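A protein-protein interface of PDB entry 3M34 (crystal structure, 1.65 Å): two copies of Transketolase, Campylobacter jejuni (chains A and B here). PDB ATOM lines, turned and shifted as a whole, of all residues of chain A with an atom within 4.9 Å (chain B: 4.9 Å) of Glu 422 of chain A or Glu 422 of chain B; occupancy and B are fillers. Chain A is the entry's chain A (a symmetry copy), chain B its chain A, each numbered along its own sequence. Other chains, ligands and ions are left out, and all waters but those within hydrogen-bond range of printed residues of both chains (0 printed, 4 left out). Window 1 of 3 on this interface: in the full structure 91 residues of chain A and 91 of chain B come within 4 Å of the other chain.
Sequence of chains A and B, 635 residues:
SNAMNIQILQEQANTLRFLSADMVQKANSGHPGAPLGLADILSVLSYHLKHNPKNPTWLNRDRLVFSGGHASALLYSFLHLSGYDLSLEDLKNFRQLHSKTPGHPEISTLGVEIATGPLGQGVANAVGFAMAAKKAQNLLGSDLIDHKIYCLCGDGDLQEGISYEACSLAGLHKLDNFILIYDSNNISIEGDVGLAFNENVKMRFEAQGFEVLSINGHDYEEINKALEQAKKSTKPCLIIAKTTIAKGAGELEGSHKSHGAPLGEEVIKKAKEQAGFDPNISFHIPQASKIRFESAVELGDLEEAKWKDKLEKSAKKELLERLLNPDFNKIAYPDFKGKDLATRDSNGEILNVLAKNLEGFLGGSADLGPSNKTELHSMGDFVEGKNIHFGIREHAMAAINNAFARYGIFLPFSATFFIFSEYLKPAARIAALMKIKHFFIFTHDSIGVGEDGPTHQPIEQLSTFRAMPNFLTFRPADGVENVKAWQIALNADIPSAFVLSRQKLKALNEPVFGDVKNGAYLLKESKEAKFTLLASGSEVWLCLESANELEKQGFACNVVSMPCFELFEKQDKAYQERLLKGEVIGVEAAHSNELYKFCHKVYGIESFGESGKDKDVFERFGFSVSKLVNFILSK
Of chain B, only Glu 422 (3.9 Å), Lys 425 (2.8 Å), Pro 426 (3.7 Å) and Arg 429 (3.6 Å) come within 4 Å of Glu 422 of chain A. Of the printed residues of chain B, Lys 425 of chain A touches Glu 422 (2.8 Å) and Glu 460 (2.7 Å). Of the printed residues of chain B, Pro 426 of chain A touches Glu 422 and Tyr 423. Of the printed residues of chain B, Glu 460 of chain A touches Lys 425 (2.7 Å) and Arg 429 (2.8 Å). Glu 422 of chain B touches just these residues of chain A: Glu 422 (3.9 Å), Lys 425 (2.8 Å), Pro 426 (3.7 Å) and Arg 429 (3.6 Å). Leu 424 of chain B touches none of the printed residues of chain A.
The side-chain carboxylate (OE1) of Glu 460 of chain B sits close to the side-chain amide nitrogen (NE2) of Gln 461 of chain B. The side-chain carboxylate (OE1) of Glu 460 of chain A sits close to the side-chain amide nitrogen (NE2) of Gln 461 of chain A, at 3.2 Å. The side-chain carboxylate (OE2) of Glu 422 of chain B is in hydrogen-bond range of the side-chain amide nitrogen (NE2) of Gln 461 of chain B (2.8 Å). The side-chain carboxylate of Glu 422 of chain A is in hydrogen-bond range of the side-chain amide nitrogen of Gln 461 of chain A (2.8 Å).
Of the 12 printed residues of chain B, 8 touch a printed residue of chain A. Hydrophobic or aromatic side chains of chain B that line the printed part of chain A: Ile 419, Tyr 423 and Pro 426. Of the 12 printed residues of chain A, 8 touch a printed residue of chain B. Among the printed residues, 17 pairs touch across the chains. Among the printed residues, Asp or Glu carboxylates within 4 Å of a Lys or Arg side-chain nitrogen of the other chain: Glu 422 of chain A with Lys 425 of chain B (2.8 Å), Lys 425 of chain A with Glu 422 of chain B (2.8 Å), Lys 425 of chain A with Glu 460 of chain B (2.7 Å), Arg 429 of chain A with Glu 460 of chain B (2.8 Å), Glu 460 of chain A with Lys 425 of chain B (2.7 Å) and Glu 460 of chain A with Arg 429 of chain B (2.8 Å).
Glu 422 of chain B touches its own counterpart, Glu 422 of chain A. Glu 422 of chain A touches Lys 425 of chain B, and with the chains exchanged Lys 425 of chain A touches Glu 422 of chain B. Lys 425 of chain A touches Glu 460 of chain B, and with the chains exchanged Glu 460 of chain A touches Lys 425 of chain B. Arg 429 of chain A touches Gln 461 of chain B, and with the chains exchanged Gln 461 of chain A touches Arg 429 of chain B. Of the 17 pairs that touch across the chains among the printed residues, 17 have their exchanged pair printed and touching as well.
Among the printed residues, merely in contact across the chains: Ile 419 of chain A with Arg 429 of chain B (3.5 Å), Glu 422 of chain A with Glu 422 of chain B (3.9 Å), Glu 422 of chain A with Pro 426 of chain B (3.7 Å), Glu 422 of chain A with Arg 429 of chain B (3.6 Å), Tyr 423 of chain A with Pro 426 of chain B (3.5 Å), Pro 426 of chain A with Glu 422 of chain B (3.7 Å), Pro 426 of chain A with Tyr 423 of chain B (3.5 Å), Arg 429 of chain A with Ile 419 of chain B (3.5 Å) and Arg 429 of chain A with Glu 422 of chain B (3.6 Å).
The guanidinium group (NE) of Arg 429 of chain A sits close to the side-chain amide nitrogen (NE2) of Gln 461 of chain B. NE of Arg 429 of chain B lies close to NE2 of Gln 461 of chain A, 3.4 Å away. The guanidinium group of Arg 429 of chain A lies within salt-bridge range of the side-chain carboxylate of Glu 460 of chain B (2.8 Å). The side-chain carboxylate of Glu 460 of chain A is in salt-bridge range of the side-chain amino group of Lys 425 of chain B (2.7 Å). The side-chain amino group (NZ) of Lys 425 of chain A is in salt-bridge range of the side-chain carboxylate (OE2) of Glu 460 of chain B (2.7 Å). The side-chain carboxylate (OE2) of Glu 460 of chain A lies within salt-bridge range of the guanidinium group (NE) of Arg 429 of chain B. NZ of Lys 425 of chain B is in salt-bridge range of OE2 of Glu 422 of chain A. The side-chain carboxylate (OE2) of Glu 422 of chain B is in salt-bridge range of the side-chain amino group (NZ) of Lys 425 of chain A (2.8 Å).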
ATOM      1  N   PHE A 418     -19.520  -5.398 -16.170  1.00  0.00           N
ATOM      2  CA  PHE A 418     -19.952  -4.908 -14.883  1.00  0.00           C
ATOM      3  C   PHE A 418     -19.591  -3.436 -14.694  1.00  0.00           C
ATOM      4  O   PHE A 418     -20.361  -2.708 -14.105  1.00  0.00           O
ATOM      5  CB  PHE A 418     -19.314  -5.762 -13.783  1.00  0.00           C
ATOM      6  CG  PHE A 418     -19.824  -5.563 -12.373  1.00  0.00           C
ATOM      7  CD1 PHE A 418     -21.125  -5.194 -12.073  1.00  0.00           C
ATOM      8  CD2 PHE A 418     -18.993  -5.856 -11.295  1.00  0.00           C
ATOM      9  CE1 PHE A 418     -21.565  -5.102 -10.783  1.00  0.00           C
ATOM     10  CE2 PHE A 418     -19.449  -5.803 -10.028  1.00  0.00           C
ATOM     11  CZ  PHE A 418     -20.722  -5.400  -9.747  1.00  0.00           C
ATOM     12  N   ILE A 419     -18.440  -2.982 -15.215  1.00  0.00           N
ATOM     13  CA  ILE A 419     -18.095  -1.543 -15.099  1.00  0.00           C
ATOM     14  C   ILE A 419     -19.186  -0.661 -15.718  1.00  0.00           C
ATOM     15  O   ILE A 419     -19.498   0.411 -15.193  1.00  0.00           O
ATOM     16  CB  ILE A 419     -16.684  -1.221 -15.650  1.00  0.00           C
ATOM     17  CG1 ILE A 419     -16.289   0.223 -15.307  1.00  0.00           C
ATOM     18  CG2 ILE A 419     -16.579  -1.534 -17.089  1.00  0.00           C
ATOM     19  CD1 ILE A 419     -16.480   0.597 -13.850  1.00  0.00           C
ATOM     20  N   PHE A 420     -19.774  -1.127 -16.830  1.00  0.00           N
ATOM     21  CA  PHE A 420     -20.788  -0.341 -17.509  1.00  0.00           C
ATOM     22  C   PHE A 420     -22.178  -0.563 -17.026  1.00  0.00           C
ATOM     23  O   PHE A 420     -23.151   0.087 -17.514  1.00  0.00           O
ATOM     24  CB  PHE A 420     -20.617  -0.402 -19.015  1.00  0.00           C
ATOM     25  CG  PHE A 420     -19.215  -0.044 -19.454  1.00  0.00           C
ATOM     26  CD1 PHE A 420     -18.603   1.077 -18.938  1.00  0.00           C
ATOM     27  CD2 PHE A 420     -18.493  -0.846 -20.296  1.00  0.00           C
ATOM     28  CE1 PHE A 420     -17.319   1.411 -19.293  1.00  0.00           C
ATOM     29  CE2 PHE A 420     -17.216  -0.508 -20.658  1.00  0.00           C
ATOM     30  CZ  PHE A 420     -16.629   0.626 -20.119  1.00  0.00           C
ATOM     31  N   SER A 421     -22.301  -1.315 -15.944  1.00  0.00           N
ATOM     32  CA  SER A 421     -23.551  -1.318 -15.177  1.00  0.00           C
ATOM     33  C   SER A 421     -23.876   0.104 -14.745  1.00  0.00           C
ATOM     34  O   SER A 421     -25.016   0.466 -14.606  1.00  0.00           O
ATOM     35  CB  SER A 421     -23.485  -2.261 -13.979  1.00  0.00           C
ATOM     36  OG  SER A 421     -22.591  -1.788 -12.978  1.00  0.00           O
ATOM     37  N   GLU A 422     -22.871   0.956 -14.526  1.00  0.00           N
ATOM     38  CA  GLU A 422     -23.107   2.324 -14.086  1.00  0.00           C
ATOM     39  C   GLU A 422     -23.943   3.126 -15.084  1.00  0.00           C
ATOM     40  O   GLU A 422     -24.577   4.089 -14.702  1.00  0.00           O
ATOM     41  CB  GLU A 422     -21.807   3.041 -13.769  1.00  0.00           C
ATOM     42  CG  GLU A 422     -21.112   2.343 -12.609  1.00  0.00           C
ATOM     43  CD  GLU A 422     -20.095   3.169 -11.874  1.00  0.00           C
ATOM     44  OE1 GLU A 422     -19.432   4.044 -12.503  1.00  0.00           O
ATOM     45  OE2 GLU A 422     -19.913   2.880 -10.644  1.00  0.00           O
ATOM     46  N   TYR A 423     -23.843   2.786 -16.364  1.00  0.00           N
ATOM     47  CA  TYR A 423     -24.588   3.473 -17.429  1.00  0.00           C
ATOM     48  C   TYR A 423     -26.066   3.140 -17.340  1.00  0.00           C
ATOM     49  O   TYR A 423     -26.880   3.947 -17.791  1.00  0.00           O
ATOM     50  CB  TYR A 423     -24.076   3.142 -18.830  1.00  0.00           C
ATOM     51  CG  TYR A 423     -22.873   3.916 -19.311  1.00  0.00           C
ATOM     52  CD1 TYR A 423     -21.628   3.794 -18.701  1.00  0.00           C
ATOM     53  CD2 TYR A 423     -22.934   4.675 -20.484  1.00  0.00           C
ATOM     54  CE1 TYR A 423     -20.542   4.466 -19.176  1.00  0.00           C
ATOM     55  CE2 TYR A 423     -21.840   5.363 -20.949  1.00  0.00           C
ATOM     56  CZ  TYR A 423     -20.652   5.236 -20.329  1.00  0.00           C
ATOM     57  OH  TYR A 423     -19.552   5.916 -20.824  1.00  0.00           O
ATOM     58  N   LEU A 424     -26.433   2.004 -16.734  1.00  0.00           N
ATOM     59  CA  LEU A 424     -27.875   1.583 -16.705  1.00  0.00           C
ATOM     60  C   LEU A 424     -28.460   1.541 -15.288  1.00  0.00           C
ATOM     61  O   LEU A 424     -29.613   1.203 -15.100  1.00  0.00           O
ATOM     62  CB  LEU A 424     -28.061   0.230 -17.406  1.00  0.00           C
ATOM     63  CG  LEU A 424     -27.190  -0.965 -16.961  1.00  0.00           C
ATOM     64  CD1 LEU A 424     -27.599  -1.360 -15.516  1.00  0.00           C
ATOM     65  CD2 LEU A 424     -27.310  -2.243 -17.945  1.00  0.00           C
ATOM     66  N   LYS A 425     -27.659   1.894 -14.287  1.00  0.00           N
ATOM     67  CA  LYS A 425     -28.105   1.802 -12.901  1.00  0.00           C
ATOM     68  C   LYS A 425     -29.456   2.521 -12.580  1.00  0.00           C
ATOM     69  O   LYS A 425     -30.255   1.982 -11.829  1.00  0.00           O
ATOM     70  CB  LYS A 425     -27.007   2.364 -11.989  1.00  0.00           C
ATOM     71  CG  LYS A 425     -27.389   2.572 -10.535  1.00  0.00           C
ATOM     72  CD  LYS A 425     -27.646   1.250  -9.751  1.00  0.00           C
ATOM     73  CE  LYS A 425     -27.958   1.558  -8.330  1.00  0.00           C
ATOM     74  NZ  LYS A 425     -29.325   2.197  -8.166  1.00  0.00           N
ATOM     75  N   PRO A 426     -29.760   3.680 -13.229  1.00  0.00           N
ATOM     76  CA  PRO A 426     -31.035   4.308 -12.870  1.00  0.00           C
ATOM     77  C   PRO A 426     -32.219   3.398 -13.273  1.00  0.00           C
ATOM     78  O   PRO A 426     -33.228   3.390 -12.575  1.00  0.00           O
ATOM     79  CB  PRO A 426     -31.002   5.671 -13.618  1.00  0.00           C
ATOM     80  CG  PRO A 426     -29.552   5.922 -13.826  1.00  0.00           C
ATOM     81  CD  PRO A 426     -28.928   4.596 -14.046  1.00  0.00           C
ATOM     82  N   ARG A 429     -32.559   0.477 -10.964  1.00  0.00           N
ATOM     83  CA  ARG A 429     -33.283   0.884  -9.769  1.00  0.00           C
ATOM     84  C   ARG A 429     -34.795   0.815  -9.938  1.00  0.00           C
ATOM     85  O   ARG A 429     -35.479   0.471  -9.057  1.00  0.00           O
ATOM     86  CB  ARG A 429     -32.885   2.306  -9.353  1.00  0.00           C
ATOM     87  CG  ARG A 429     -33.175   2.662  -7.913  1.00  0.00           C
ATOM     88  CD  ARG A 429     -32.665   4.060  -7.523  1.00  0.00           C
ATOM     89  NE  ARG A 429     -32.591   4.219  -6.097  1.00  0.00           N
ATOM     90  CZ  ARG A 429     -33.482   4.821  -5.347  1.00  0.00           C
ATOM     91  NH1 ARG A 429     -34.552   5.378  -5.859  1.00  0.00           N
ATOM     92  NH2 ARG A 429     -33.259   4.865  -4.060  1.00  0.00           N
ATOM     93  N   GLU A 460     -16.095  -0.341  -7.114  1.00  0.00           N
ATOM     94  CA  GLU A 460     -17.217   0.065  -6.276  1.00  0.00           C
ATOM     95  C   GLU A 460     -18.587  -0.488  -6.660  1.00  0.00           C
ATOM     96  O   GLU A 460     -19.552  -0.251  -5.939  1.00  0.00           O
ATOM     97  CB  GLU A 460     -17.247   1.577  -6.148  1.00  0.00           C
ATOM     98  CG  GLU A 460     -17.674   2.353  -7.465  1.00  0.00           C
ATOM     99  CD  GLU A 460     -16.588   2.561  -8.472  1.00  0.00           C
ATOM    100  OE1 GLU A 460     -15.660   1.748  -8.622  1.00  0.00           O
ATOM    101  OE2 GLU A 460     -16.703   3.595  -9.213  1.00  0.00           O
ATOM    102  N   GLN A 461     -18.692  -1.209  -7.791  1.00  0.00           N
ATOM    103  CA  GLN A 461     -19.995  -1.567  -8.334  1.00  0.00           C
ATOM    104  C   GLN A 461     -20.666  -2.644  -7.494  1.00  0.00           C
ATOM    105  O   GLN A 461     -21.887  -2.635  -7.273  1.00  0.00           O
ATOM    106  CB  GLN A 461     -19.882  -1.968  -9.809  1.00  0.00           C
ATOM    107  CG  GLN A 461     -19.550  -0.794 -10.693  1.00  0.00           C
ATOM    108  CD  GLN A 461     -18.101  -0.290 -10.553  1.00  0.00           C
ATOM    109  OE1 GLN A 461     -17.183  -1.055 -10.276  1.00  0.00           O
ATOM    110  NE2 GLN A 461     -17.879   0.992 -10.856  1.00  0.00           N
ATOM    111  N   PHE B 418     -29.474  14.301  -5.535  1.00  0.00           N
ATOM    112  CA  PHE B 418     -28.591  13.193  -5.257  1.00  0.00           C
ATOM    113  C   PHE B 418     -29.086  11.904  -5.910  1.00  0.00           C
ATOM    114  O   PHE B 418     -28.279  11.125  -6.370  1.00  0.00           O
ATOM    115  CB  PHE B 418     -28.476  13.015  -3.740  1.00  0.00           C
ATOM    116  CG  PHE B 418     -27.414  12.061  -3.237  1.00  0.00           C
ATOM    117  CD1 PHE B 418     -26.216  11.832  -3.892  1.00  0.00           C
ATOM    118  CD2 PHE B 418     -27.579  11.442  -2.001  1.00  0.00           C
ATOM    119  CE1 PHE B 418     -25.252  11.023  -3.362  1.00  0.00           C
ATOM    120  CE2 PHE B 418     -26.605  10.679  -1.468  1.00  0.00           C
ATOM    121  CZ  PHE B 418     -25.446  10.432  -2.144  1.00  0.00           C
ATOM    122  N   ILE B 419     -30.408  11.685  -5.984  1.00  0.00           N
ATOM    123  CA  ILE B 419     -30.917  10.471  -6.669  1.00  0.00           C
ATOM    124  C   ILE B 419     -30.421  10.404  -8.119  1.00  0.00           C
ATOM    125  O   ILE B 419     -30.103   9.324  -8.624  1.00  0.00           O
ATOM    126  CB  ILE B 419     -32.455  10.321  -6.557  1.00  0.00           C
ATOM    127  CG1 ILE B 419     -32.902   8.949  -7.083  1.00  0.00           C
ATOM    128  CG2 ILE B 419     -33.157  11.453  -7.194  1.00  0.00           C
ATOM    129  CD1 ILE B 419     -32.127   7.776  -6.513  1.00  0.00           C
ATOM    130  N   PHE B 420     -30.344  11.569  -8.779  1.00  0.00           N
ATOM    131  CA  PHE B 420     -29.926  11.599 -10.169  1.00  0.00           C
ATOM    132  C   PHE B 420     -28.457  11.712 -10.377  1.00  0.00           C
ATOM    133  O   PHE B 420     -27.960  11.715 -11.544  1.00  0.00           O
ATOM    134  CB  PHE B 420     -30.763  12.573 -10.977  1.00  0.00           C
ATOM    135  CG  PHE B 420     -32.247  12.326 -10.823  1.00  0.00           C
ATOM    136  CD1 PHE B 420     -32.742  11.047 -10.935  1.00  0.00           C
ATOM    137  CD2 PHE B 420     -33.116  13.331 -10.494  1.00  0.00           C
ATOM    138  CE1 PHE B 420     -34.081  10.787 -10.769  1.00  0.00           C
ATOM    139  CE2 PHE B 420     -34.453  13.075 -10.338  1.00  0.00           C
ATOM    140  CZ  PHE B 420     -34.919  11.774 -10.456  1.00  0.00           C
ATOM    141  N   SER B 421     -27.708  11.609  -9.290  1.00  0.00           N
ATOM    142  CA  SER B 421     -26.269  11.352  -9.398  1.00  0.00           C
ATOM    143  C   SER B 421     -26.047  10.071 -10.188  1.00  0.00           C
ATOM    144  O   SER B 421     -25.062   9.921 -10.864  1.00  0.00           O
ATOM    145  CB  SER B 421     -25.596  11.283  -8.030  1.00  0.00           C
ATOM    146  OG  SER B 421     -25.992  10.127  -7.299  1.00  0.00           O
ATOM    147  N   GLU B 422     -26.972   9.110 -10.130  1.00  0.00           N
ATOM    148  CA  GLU B 422     -26.814   7.848 -10.840  1.00  0.00           C
ATOM    149  C   GLU B 422     -26.701   8.037 -12.353  1.00  0.00           C
ATOM    150  O   GLU B 422     -26.151   7.188 -13.026  1.00  0.00           O
ATOM    151  CB  GLU B 422     -27.925   6.872 -10.497  1.00  0.00           C
ATOM    152  CG  GLU B 422     -27.859   6.527  -9.016  1.00  0.00           C
ATOM    153  CD  GLU B 422     -28.549   5.254  -8.617  1.00  0.00           C
ATOM    154  OE1 GLU B 422     -29.576   4.879  -9.253  1.00  0.00           O
ATOM    155  OE2 GLU B 422     -28.082   4.654  -7.591  1.00  0.00           O
ATOM    156  N   TYR B 423     -27.320   9.088 -12.877  1.00  0.00           N
ATOM    157  CA  TYR B 423     -27.297   9.388 -14.316  1.00  0.00           C
ATOM    158  C   TYR B 423     -25.914   9.852 -14.737  1.00  0.00           C
ATOM    159  O   TYR B 423     -25.567   9.685 -15.906  1.00  0.00           O
ATOM    160  CB  TYR B 423     -28.331  10.435 -14.728  1.00  0.00           C
ATOM    161  CG  TYR B 423     -29.739   9.941 -14.958  1.00  0.00           C
ATOM    162  CD1 TYR B 423     -30.510   9.416 -13.926  1.00  0.00           C
ATOM    163  CD2 TYR B 423     -30.370  10.131 -16.192  1.00  0.00           C
ATOM    164  CE1 TYR B 423     -31.795   9.016 -14.141  1.00  0.00           C
ATOM    165  CE2 TYR B 423     -31.660   9.711 -16.406  1.00  0.00           C
ATOM    166  CZ  TYR B 423     -32.378   9.194 -15.392  1.00  0.00           C
ATOM    167  OH  TYR B 423     -33.686   8.798 -15.618  1.00  0.00           O
ATOM    168  N   LEU B 424     -25.106  10.385 -13.811  1.00  0.00           N
ATOM    169  CA  LEU B 424     -23.766  10.945 -14.195  1.00  0.00           C
ATOM    170  C   LEU B 424     -22.593  10.182 -13.570  1.00  0.00           C
ATOM    171  O   LEU B 424     -21.446  10.527 -13.774  1.00  0.00           O
ATOM    172  CB  LEU B 424     -23.683  12.440 -13.851  1.00  0.00           C
ATOM    173  CG  LEU B 424     -24.011  12.891 -12.412  1.00  0.00           C
ATOM    174  CD1 LEU B 424     -22.913  12.342 -11.462  1.00  0.00           C
ATOM    175  CD2 LEU B 424     -24.131  14.497 -12.258  1.00  0.00           C
ATOM    176  N   LYS B 425     -22.886   9.133 -12.806  1.00  0.00           N
ATOM    177  CA  LYS B 425     -21.839   8.401 -12.102  1.00  0.00           C
ATOM    178  C   LYS B 425     -20.651   7.906 -12.991  1.00  0.00           C
ATOM    179  O   LYS B 425     -19.511   7.978 -12.558  1.00  0.00           O
ATOM    180  CB  LYS B 425     -22.469   7.198 -11.389  1.00  0.00           C
ATOM    181  CG  LYS B 425     -21.500   6.186 -10.805  1.00  0.00           C
ATOM    182  CD  LYS B 425     -20.670   6.724  -9.600  1.00  0.00           C
ATOM    183  CE  LYS B 425     -19.796   5.645  -9.068  1.00  0.00           C
ATOM    184  NZ  LYS B 425     -18.652   5.313 -10.010  1.00  0.00           N
ATOM    185  N   PRO B 426     -20.902   7.507 -14.270  1.00  0.00           N
ATOM    186  CA  PRO B 426     -19.746   7.042 -15.042  1.00  0.00           C
ATOM    187  C   PRO B 426     -18.741   8.197 -15.261  1.00  0.00           C
ATOM    188  O   PRO B 426     -17.541   7.944 -15.296  1.00  0.00           O
ATOM    189  CB  PRO B 426     -20.372   6.492 -16.355  1.00  0.00           C
ATOM    190  CG  PRO B 426     -21.771   6.171 -15.968  1.00  0.00           C
ATOM    191  CD  PRO B 426     -22.171   7.189 -14.969  1.00  0.00           C
ATOM    192  N   ARG B 429     -16.837   8.977 -12.139  1.00  0.00           N
ATOM    193  CA  ARG B 429     -15.729   8.043 -12.000  1.00  0.00           C
ATOM    194  C   ARG B 429     -14.486   8.480 -12.763  1.00  0.00           C
ATOM    195  O   ARG B 429     -13.420   8.302 -12.320  1.00  0.00           O
ATOM    196  CB  ARG B 429     -16.141   6.641 -12.464  1.00  0.00           C
ATOM    197  CG  ARG B 429     -15.286   5.511 -11.941  1.00  0.00           C
ATOM    198  CD  ARG B 429     -15.803   4.121 -12.354  1.00  0.00           C
ATOM    199  NE  ARG B 429     -15.233   3.081 -11.544  1.00  0.00           N
ATOM    200  CZ  ARG B 429     -14.222   2.316 -11.880  1.00  0.00           C
ATOM    201  NH1 ARG B 429     -13.636   2.421 -13.048  1.00  0.00           N
ATOM    202  NH2 ARG B 429     -13.826   1.422 -11.013  1.00  0.00           N
ATOM    203  N   GLU B 460     -29.156   4.118  -1.594  1.00  0.00           N
ATOM    204  CA  GLU B 460     -27.870   3.485  -1.859  1.00  0.00           C
ATOM    205  C   GLU B 460     -26.760   4.396  -2.381  1.00  0.00           C
ATOM    206  O   GLU B 460     -25.633   3.936  -2.537  1.00  0.00           O
ATOM    207  CB  GLU B 460     -28.061   2.277  -2.758  1.00  0.00           C
ATOM    208  CG  GLU B 460     -28.447   2.613  -4.261  1.00  0.00           C
ATOM    209  CD  GLU B 460     -29.893   2.900  -4.508  1.00  0.00           C
ATOM    210  OE1 GLU B 460     -30.617   3.434  -3.650  1.00  0.00           O
ATOM    211  OE2 GLU B 460     -30.328   2.619  -5.675  1.00  0.00           O
ATOM    212  N   GLN B 461     -27.063   5.676  -2.666  1.00  0.00           N
ATOM    213  CA  GLN B 461     -26.121   6.528  -3.378  1.00  0.00           C
ATOM    214  C   GLN B 461     -24.952   6.923  -2.487  1.00  0.00           C
ATOM    215  O   GLN B 461     -23.794   6.999  -2.925  1.00  0.00           O
ATOM    216  CB  GLN B 461     -26.832   7.747  -3.976  1.00  0.00           C
ATOM    217  CG  GLN B 461     -27.745   7.370  -5.114  1.00  0.00           C
ATOM    218  CD  GLN B 461     -29.028   6.638  -4.675  1.00  0.00           C
ATOM    219  OE1 GLN B 461     -29.553   6.866  -3.590  1.00  0.00           O
ATOM    220  NE2 GLN B 461     -29.597   5.830  -5.574  1.00  0.00           N
